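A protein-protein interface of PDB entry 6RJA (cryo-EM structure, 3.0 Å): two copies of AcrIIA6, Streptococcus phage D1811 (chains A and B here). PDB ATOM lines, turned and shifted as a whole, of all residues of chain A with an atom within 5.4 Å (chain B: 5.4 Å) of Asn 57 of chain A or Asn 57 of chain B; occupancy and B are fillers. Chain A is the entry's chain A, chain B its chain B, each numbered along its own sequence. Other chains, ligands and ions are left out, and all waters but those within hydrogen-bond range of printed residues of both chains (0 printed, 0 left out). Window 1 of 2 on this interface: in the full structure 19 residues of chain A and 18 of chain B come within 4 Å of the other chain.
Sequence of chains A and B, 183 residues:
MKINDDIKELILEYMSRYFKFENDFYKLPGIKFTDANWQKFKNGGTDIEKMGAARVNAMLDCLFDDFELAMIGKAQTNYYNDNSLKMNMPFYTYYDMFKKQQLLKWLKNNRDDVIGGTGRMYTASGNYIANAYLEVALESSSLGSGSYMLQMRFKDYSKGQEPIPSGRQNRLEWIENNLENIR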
ATOM      1  N   MET A   1     -20.157  -8.929  13.576  1.00  0.00           N
ATOM      2  CA  MET A   1     -19.315  -8.835  12.388  1.00  0.00           C
ATOM      3  C   MET A   1     -18.012  -9.607  12.569  1.00  0.00           C
ATOM      4  O   MET A   1     -17.925 -10.519  13.385  1.00  0.00           O
ATOM      5  CB  MET A   1     -19.019  -7.371  12.060  1.00  0.00           C
ATOM      6  CG  MET A   1     -18.435  -6.580  13.218  1.00  0.00           C
ATOM      7  SD  MET A   1     -17.845  -4.961  12.708  1.00  0.00           S
ATOM      8  CE  MET A   1     -19.398  -4.178  12.304  1.00  0.00           C
ATOM      9  N   ILE A   3     -13.827  -8.842  13.197  1.00  0.00           N
ATOM     10  CA  ILE A   3     -12.845  -7.844  13.605  1.00  0.00           C
ATOM     11  C   ILE A   3     -11.483  -8.291  13.093  1.00  0.00           C
ATOM     12  O   ILE A   3     -10.985  -9.349  13.493  1.00  0.00           O
ATOM     13  CB  ILE A   3     -12.825  -7.665  15.130  1.00  0.00           C
ATOM     14  CG1 ILE A   3     -14.246  -7.512  15.671  1.00  0.00           C
ATOM     15  CG2 ILE A   3     -11.962  -6.489  15.520  1.00  0.00           C
ATOM     16  CD1 ILE A   3     -14.875  -6.171  15.423  1.00  0.00           C
ATOM     17  N   GLY A  52      -9.984  -5.090  24.192  1.00  0.00           N
ATOM     18  CA  GLY A  52     -11.246  -5.202  24.886  1.00  0.00           C
ATOM     19  C   GLY A  52     -12.409  -5.118  23.921  1.00  0.00           C
ATOM     20  O   GLY A  52     -12.343  -4.452  22.894  1.00  0.00           O
ATOM     21  N   ALA A  53     -13.490  -5.824  24.250  1.00  0.00           N
ATOM     22  CA  ALA A  53     -14.655  -5.816  23.373  1.00  0.00           C
ATOM     23  C   ALA A  53     -15.392  -4.488  23.455  1.00  0.00           C
ATOM     24  O   ALA A  53     -15.853  -3.958  22.433  1.00  0.00           O
ATOM     25  CB  ALA A  53     -15.584  -6.973  23.724  1.00  0.00           C
ATOM     26  N   ALA A  54     -15.468  -3.914  24.658  1.00  0.00           N
ATOM     27  CA  ALA A  54     -16.205  -2.675  24.853  1.00  0.00           C
ATOM     28  C   ALA A  54     -15.521  -1.486  24.191  1.00  0.00           C
ATOM     29  O   ALA A  54     -16.205  -0.587  23.699  1.00  0.00           O
ATOM     30  CB  ALA A  54     -16.394  -2.418  26.343  1.00  0.00           C
ATOM     31  N   ARG A  55     -14.187  -1.490  24.103  1.00  0.00           N
ATOM     32  CA  ARG A  55     -13.482  -0.366  23.489  1.00  0.00           C
ATOM     33  C   ARG A  55     -13.653  -0.345  21.974  1.00  0.00           C
ATOM     34  O   ARG A  55     -13.912   0.716  21.390  1.00  0.00           O
ATOM     35  CB  ARG A  55     -12.001  -0.415  23.847  1.00  0.00           C
ATOM     36  CG  ARG A  55     -11.688   0.061  25.245  1.00  0.00           C
ATOM     37  CD  ARG A  55     -10.209  -0.061  25.530  1.00  0.00           C
ATOM     38  NE  ARG A  55      -9.503   1.199  25.351  1.00  0.00           N
ATOM     39  CZ  ARG A  55      -8.204   1.290  25.101  1.00  0.00           C
ATOM     40  NH1 ARG A  55      -7.471   0.195  24.989  1.00  0.00           N
ATOM     41  NH2 ARG A  55      -7.639   2.474  24.953  1.00  0.00           N
ATOM     42  N   VAL A  56     -13.510  -1.502  21.322  1.00  0.00           N
ATOM     43  CA  VAL A  56     -13.684  -1.562  19.876  1.00  0.00           C
ATOM     44  C   VAL A  56     -15.142  -1.326  19.505  1.00  0.00           C
ATOM     45  O   VAL A  56     -15.444  -0.661  18.501  1.00  0.00           O
ATOM     46  CB  VAL A  56     -13.167  -2.904  19.330  1.00  0.00           C
ATOM     47  CG1 VAL A  56     -13.081  -2.862  17.827  1.00  0.00           C
ATOM     48  CG2 VAL A  56     -11.811  -3.201  19.896  1.00  0.00           C
ATOM     49  N   ASN A  57     -16.070  -1.821  20.328  1.00  0.00           N
ATOM     50  CA  ASN A  57     -17.473  -1.532  20.074  1.00  0.00           C
ATOM     51  C   ASN A  57     -17.810  -0.065  20.316  1.00  0.00           C
ATOM     52  O   ASN A  57     -18.672   0.480  19.626  1.00  0.00           O
ATOM     53  CB  ASN A  57     -18.358  -2.443  20.918  1.00  0.00           C
ATOM     54  CG  ASN A  57     -18.588  -3.788  20.266  1.00  0.00           C
ATOM     55  OD1 ASN A  57     -18.087  -4.807  20.725  1.00  0.00           O
ATOM     56  ND2 ASN A  57     -19.349  -3.795  19.185  1.00  0.00           N
ATOM     57  N   ALA A  58     -17.107   0.609  21.231  1.00  0.00           N
ATOM     58  CA  ALA A  58     -17.327   2.040  21.422  1.00  0.00           C
ATOM     59  C   ALA A  58     -16.794   2.860  20.253  1.00  0.00           C
ATOM     60  O   ALA A  58     -17.425   3.843  19.847  1.00  0.00           O
ATOM     61  CB  ALA A  58     -16.689   2.499  22.730  1.00  0.00           C
ATOM     62  N   MET A  59     -15.642   2.469  19.697  1.00  0.00           N
ATOM     63  CA  MET A  59     -15.115   3.150  18.512  1.00  0.00           C
ATOM     64  C   MET A  59     -16.048   2.993  17.314  1.00  0.00           C
ATOM     65  O   MET A  59     -16.364   3.974  16.620  1.00  0.00           O
ATOM     66  CB  MET A  59     -13.726   2.618  18.165  1.00  0.00           C
ATOM     67  CG  MET A  59     -12.658   2.908  19.198  1.00  0.00           C
ATOM     68  SD  MET A  59     -11.001   2.919  18.496  1.00  0.00           S
ATOM     69  CE  MET A  59     -10.568   1.194  18.593  1.00  0.00           C
ATOM     70  N   LEU A  60     -16.518   1.765  17.073  1.00  0.00           N
ATOM     71  CA  LEU A  60     -17.441   1.527  15.967  1.00  0.00           C
ATOM     72  C   LEU A  60     -18.791   2.196  16.192  1.00  0.00           C
ATOM     73  O   LEU A  60     -19.424   2.638  15.231  1.00  0.00           O
ATOM     74  CB  LEU A  60     -17.622   0.028  15.752  1.00  0.00           C
ATOM     75  CG  LEU A  60     -16.463  -0.725  15.105  1.00  0.00           C
ATOM     76  CD1 LEU A  60     -16.695  -2.216  15.197  1.00  0.00           C
ATOM     77  CD2 LEU A  60     -16.299  -0.306  13.665  1.00  0.00           C
ATOM     78  N   ASP A  61     -19.243   2.289  17.445  1.00  0.00           N
ATOM     79  CA  ASP A  61     -20.501   2.959  17.745  1.00  0.00           C
ATOM     80  C   ASP A  61     -20.382   4.467  17.569  1.00  0.00           C
ATOM     81  O   ASP A  61     -21.352   5.119  17.170  1.00  0.00           O
ATOM     82  CB  ASP A  61     -20.913   2.605  19.175  1.00  0.00           C
ATOM     83  CG  ASP A  61     -22.395   2.818  19.459  1.00  0.00           C
ATOM     84  OD1 ASP A  61     -23.065   3.651  18.825  1.00  0.00           O
ATOM     85  OD2 ASP A  61     -22.909   2.126  20.360  1.00  0.00           O
ATOM     86  N   CYS A  62     -19.208   5.044  17.833  1.00  0.00           N
ATOM     87  CA  CYS A  62     -19.062   6.478  17.606  1.00  0.00           C
ATOM     88  C   CYS A  62     -19.006   6.801  16.125  1.00  0.00           C
ATOM     89  O   CYS A  62     -19.641   7.760  15.678  1.00  0.00           O
ATOM     90  CB  CYS A  62     -17.823   7.025  18.306  1.00  0.00           C
ATOM     91  SG  CYS A  62     -17.697   8.831  18.192  1.00  0.00           S
ATOM     92  N   MET B   1     -22.481  -1.149  19.402  1.00  0.00           N
ATOM     93  CA  MET B   1     -23.425  -1.220  20.513  1.00  0.00           C
ATOM     94  C   MET B   1     -22.726  -0.994  21.850  1.00  0.00           C
ATOM     95  O   MET B   1     -21.658  -0.393  21.911  1.00  0.00           O
ATOM     96  CB  MET B   1     -24.143  -2.570  20.516  1.00  0.00           C
ATOM     97  CG  MET B   1     -23.212  -3.771  20.502  1.00  0.00           C
ATOM     98  SD  MET B   1     -24.085  -5.315  20.791  1.00  0.00           S
ATOM     99  CE  MET B   1     -25.046  -5.412  19.289  1.00  0.00           C
ATOM    100  N   ILE B   3     -21.503  -3.232  25.312  1.00  0.00           N
ATOM    101  CA  ILE B   3     -21.243  -4.567  25.840  1.00  0.00           C
ATOM    102  C   ILE B   3     -21.276  -4.483  27.358  1.00  0.00           C
ATOM    103  O   ILE B   3     -20.455  -3.784  27.962  1.00  0.00           O
ATOM    104  CB  ILE B   3     -19.895  -5.112  25.349  1.00  0.00           C
ATOM    105  CG1 ILE B   3     -19.752  -4.915  23.841  1.00  0.00           C
ATOM    106  CG2 ILE B   3     -19.736  -6.567  25.728  1.00  0.00           C
ATOM    107  CD1 ILE B   3     -20.554  -5.867  22.999  1.00  0.00           C
ATOM    108  N   GLY B  52     -11.791 -10.637  24.560  1.00  0.00           N
ATOM    109  CA  GLY B  52     -11.385 -10.289  23.217  1.00  0.00           C
ATOM    110  C   GLY B  52     -12.551  -9.742  22.420  1.00  0.00           C
ATOM    111  O   GLY B  52     -13.700 -10.116  22.626  1.00  0.00           O
ATOM    112  N   ALA B  53     -12.247  -8.822  21.504  1.00  0.00           N
ATOM    113  CA  ALA B  53     -13.308  -8.226  20.699  1.00  0.00           C
ATOM    114  C   ALA B  53     -13.825  -9.213  19.662  1.00  0.00           C
ATOM    115  O   ALA B  53     -15.038  -9.289  19.416  1.00  0.00           O
ATOM    116  CB  ALA B  53     -12.804  -6.951  20.030  1.00  0.00           C
ATOM    117  N   ALA B  54     -12.922 -10.006  19.083  1.00  0.00           N
ATOM    118  CA  ALA B  54     -13.307 -10.938  18.034  1.00  0.00           C
ATOM    119  C   ALA B  54     -14.159 -12.085  18.565  1.00  0.00           C
ATOM    120  O   ALA B  54     -15.052 -12.555  17.858  1.00  0.00           O
ATOM    121  CB  ALA B  54     -12.060 -11.478  17.344  1.00  0.00           C
ATOM    122  N   ARG B  55     -13.952 -12.501  19.818  1.00  0.00           N
ATOM    123  CA  ARG B  55     -14.735 -13.607  20.369  1.00  0.00           C
ATOM    124  C   ARG B  55     -16.171 -13.194  20.667  1.00  0.00           C
ATOM    125  O   ARG B  55     -17.112 -13.931  20.340  1.00  0.00           O
ATOM    126  CB  ARG B  55     -14.072 -14.141  21.633  1.00  0.00           C
ATOM    127  CG  ARG B  55     -12.873 -15.024  21.377  1.00  0.00           C
ATOM    128  CD  ARG B  55     -12.255 -15.473  22.681  1.00  0.00           C
ATOM    129  NE  ARG B  55     -12.681 -16.811  23.065  1.00  0.00           N
ATOM    130  CZ  ARG B  55     -12.663 -17.261  24.312  1.00  0.00           C
ATOM    131  NH1 ARG B  55     -12.250 -16.480  25.296  1.00  0.00           N
ATOM    132  NH2 ARG B  55     -13.067 -18.490  24.578  1.00  0.00           N
ATOM    133  N   VAL B  56     -16.362 -12.028  21.287  1.00  0.00           N
ATOM    134  CA  VAL B  56     -17.711 -11.558  21.582  1.00  0.00           C
ATOM    135  C   VAL B  56     -18.441 -11.199  20.295  1.00  0.00           C
ATOM    136  O   VAL B  56     -19.648 -11.456  20.155  1.00  0.00           O
ATOM    137  CB  VAL B  56     -17.664 -10.373  22.561  1.00  0.00           C
ATOM    138  CG1 VAL B  56     -19.041 -10.068  23.086  1.00  0.00           C
ATOM    139  CG2 VAL B  56     -16.754 -10.691  23.710  1.00  0.00           C
ATOM    140  N   ASN B  57     -17.721 -10.644  19.318  1.00  0.00           N
ATOM    141  CA  ASN B  57     -18.350 -10.379  18.032  1.00  0.00           C
ATOM    142  C   ASN B  57     -18.680 -11.664  17.280  1.00  0.00           C
ATOM    143  O   ASN B  57     -19.678 -11.704  16.559  1.00  0.00           O
ATOM    144  CB  ASN B  57     -17.465  -9.465  17.193  1.00  0.00           C
ATOM    145  CG  ASN B  57     -17.674  -8.003  17.518  1.00  0.00           C
ATOM    146  OD1 ASN B  57     -16.810  -7.354  18.095  1.00  0.00           O
ATOM    147  ND2 ASN B  57     -18.829  -7.478  17.148  1.00  0.00           N
ATOM    148  N   ALA B  58     -17.908 -12.736  17.479  1.00  0.00           N
ATOM    149  CA  ALA B  58     -18.249 -14.013  16.857  1.00  0.00           C
ATOM    150  C   ALA B  58     -19.479 -14.648  17.495  1.00  0.00           C
ATOM    151  O   ALA B  58     -20.309 -15.234  16.790  1.00  0.00           O
ATOM    152  CB  ALA B  58     -17.060 -14.965  16.931  1.00  0.00           C
ATOM    153  N   MET B  59     -19.615 -14.536  18.821  1.00  0.00           N
ATOM    154  CA  MET B  59     -20.816 -15.038  19.494  1.00  0.00           C
ATOM    155  C   MET B  59     -22.067 -14.291  19.039  1.00  0.00           C
ATOM    156  O   MET B  59     -23.095 -14.907  18.714  1.00  0.00           O
ATOM    157  CB  MET B  59     -20.662 -14.928  21.010  1.00  0.00           C
ATOM    158  CG  MET B  59     -19.579 -15.801  21.604  1.00  0.00           C
ATOM    159  SD  MET B  59     -19.875 -16.187  23.338  1.00  0.00           S
ATOM    160  CE  MET B  59     -19.127 -14.783  24.140  1.00  0.00           C
ATOM    161  N   LEU B  60     -21.988 -12.957  18.991  1.00  0.00           N
ATOM    162  CA  LEU B  60     -23.124 -12.161  18.540  1.00  0.00           C
ATOM    163  C   LEU B  60     -23.425 -12.378  17.061  1.00  0.00           C
ATOM    164  O   LEU B  60     -24.591 -12.334  16.660  1.00  0.00           O
ATOM    165  CB  LEU B  60     -22.870 -10.683  18.814  1.00  0.00           C
ATOM    166  CG  LEU B  60     -22.971 -10.221  20.266  1.00  0.00           C
ATOM    167  CD1 LEU B  60     -22.448  -8.809  20.400  1.00  0.00           C
ATOM    168  CD2 LEU B  60     -24.397 -10.302  20.749  1.00  0.00           C
ATOM    169  N   ASP B  61     -22.402 -12.623  16.242  1.00  0.00           N
ATOM    170  CA  ASP B  61     -22.613 -12.891  14.826  1.00  0.00           C
ATOM    171  C   ASP B  61     -23.244 -14.260  14.609  1.00  0.00           C
ATOM    172  O   ASP B  61     -24.032 -14.434  13.674  1.00  0.00           O
ATOM    173  CB  ASP B  61     -21.269 -12.785  14.103  1.00  0.00           C
ATOM    174  CG  ASP B  61     -21.396 -12.558  12.600  1.00  0.00           C
ATOM    175  OD1 ASP B  61     -22.395 -12.938  11.967  1.00  0.00           O
ATOM    176  OD2 ASP B  61     -20.450 -11.980  12.029  1.00  0.00           O
ATOM    177  N   CYS B  62     -22.937 -15.240  15.462  1.00  0.00           N
ATOM    178  CA  CYS B  62     -23.585 -16.537  15.303  1.00  0.00           C
ATOM    179  C   CYS B  62     -25.043 -16.485  15.724  1.00  0.00           C
ATOM    180  O   CYS B  62     -25.905 -17.037  15.034  1.00  0.00           O
ATOM    181  CB  CYS B  62     -22.855 -17.619  16.091  1.00  0.00           C
ATOM    182  SG  CYS B  62     -23.524 -19.276  15.787  1.00  0.00           S
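Asn 57 of chain A touches just these residues of chain B: Met 1 (3.9 Å), Ile 3 (3.5 Å) and Asn 57 (3.9 Å). Asn 57 of chain B touches just these residues of chain A: Met 1 (3.8 Å), Ile 3 (3.5 Å) and Asn 57 (3.9 Å). Printed residues of chain A within 4 Å of Met 1 of chain B: Asn 57 and Asp 61. Printed residues of chain B within 4 Å of Asp 61 of chain A: Met 1 (3.2 Å). The nearest printed residue of chain B that does not touch Asn 57 of chain A is Ala 53 of chain B (5.6 Å).
O of Met 1 of chain A touches O of Asn 57 of chain B, 3.8 Å away. Ile 3 of chain A touches Asn 57 of chain B. O of Gly 52 of chain A touches CB of Ala 53 of chain B (3.8 Å). Gly 52 of chain B touches Ala 53 of chain A (O to CB, 3.8 Å). Ala 53 of chain A touches Ala 53 of chain B. Val 56 of chain B touches Ala 53 of chain A (CG2 to CB, 3.9 Å). CB of Ala 53 of chain B touches CG2 of Val 56 of chain A, at 3.9 Å. O of Met 1 of chain B touches O of Asn 57 of chain A, at 3.9 Å. Ile 3 of chain B touches Asn 57 of chain A. OD1 of Asn 57 of chain B touches OD1 of Asn 57 of chain A, at 3.9 Å.
Hydrophobic or aromatic side chains of chain B within 4 Å of the printed part of chain A: Ile 3, Ala 53 and Val 56. Of the 13 printed residues of chain A, 7 touch a printed residue of chain B. Printed residues of chain A that touch a printed residue of chain B: Met 1, Ile 3, Gly 52, Ala 53, Val 56, Asn 57 and Asp 61. Hydrophobic or aromatic side chains of chain A within 4 Å of the printed part of chain B: Ile 3, Ala 53 and Val 56. Among the printed residues, 12 pairs touch across the chains. Among the printed residues, no Asp or Glu carboxylate lies within 4 Å of a Lys or Arg side-chain nitrogen of the other chain.
The backbone carbonyl oxygen (O) of Ala 53 of chain B sits close to the side-chain amide oxygen (OD1) of Asn 57 of chain B (2.9 Å). The backbone carbonyl oxygen (O) of Ala 53 of chain A sits close to the side-chain amide oxygen (OD1) of Asn 57 of chain A (2.9 Å).
Met 1 of chain A touches Asn 57 of chain B, and with the chains exchanged Asn 57 of chain A touches Met 1 of chain B. Gly 52 of chain A touches Ala 53 of chain B, and with the chains exchanged Ala 53 of chain A touches Gly 52 of chain B. Ala 53 of chain A touches Val 56 of chain B, and with the chains exchanged Val 56 of chain A touches Ala 53 of chain B. Asn 57 of chain B touches its own counterpart, Asn 57 of chain A. Positions printed for both chains: 1, 3, 52, 53, 54, 55, 56, 57, 58, 59, 60, 61 and 62. Of the 12 pairs that touch across the chains among the printed residues, 12 have their exchanged pair printed and touching as well.
The side-chain carboxylate of Asp 61 of chain A sits close to the backbone NH of Met 1 of chain B. The backbone NH (N) of Met 1 of chain A sits close to the side-chain carboxylate (OD2) of Asp 61 of chain B (3.4 Å).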
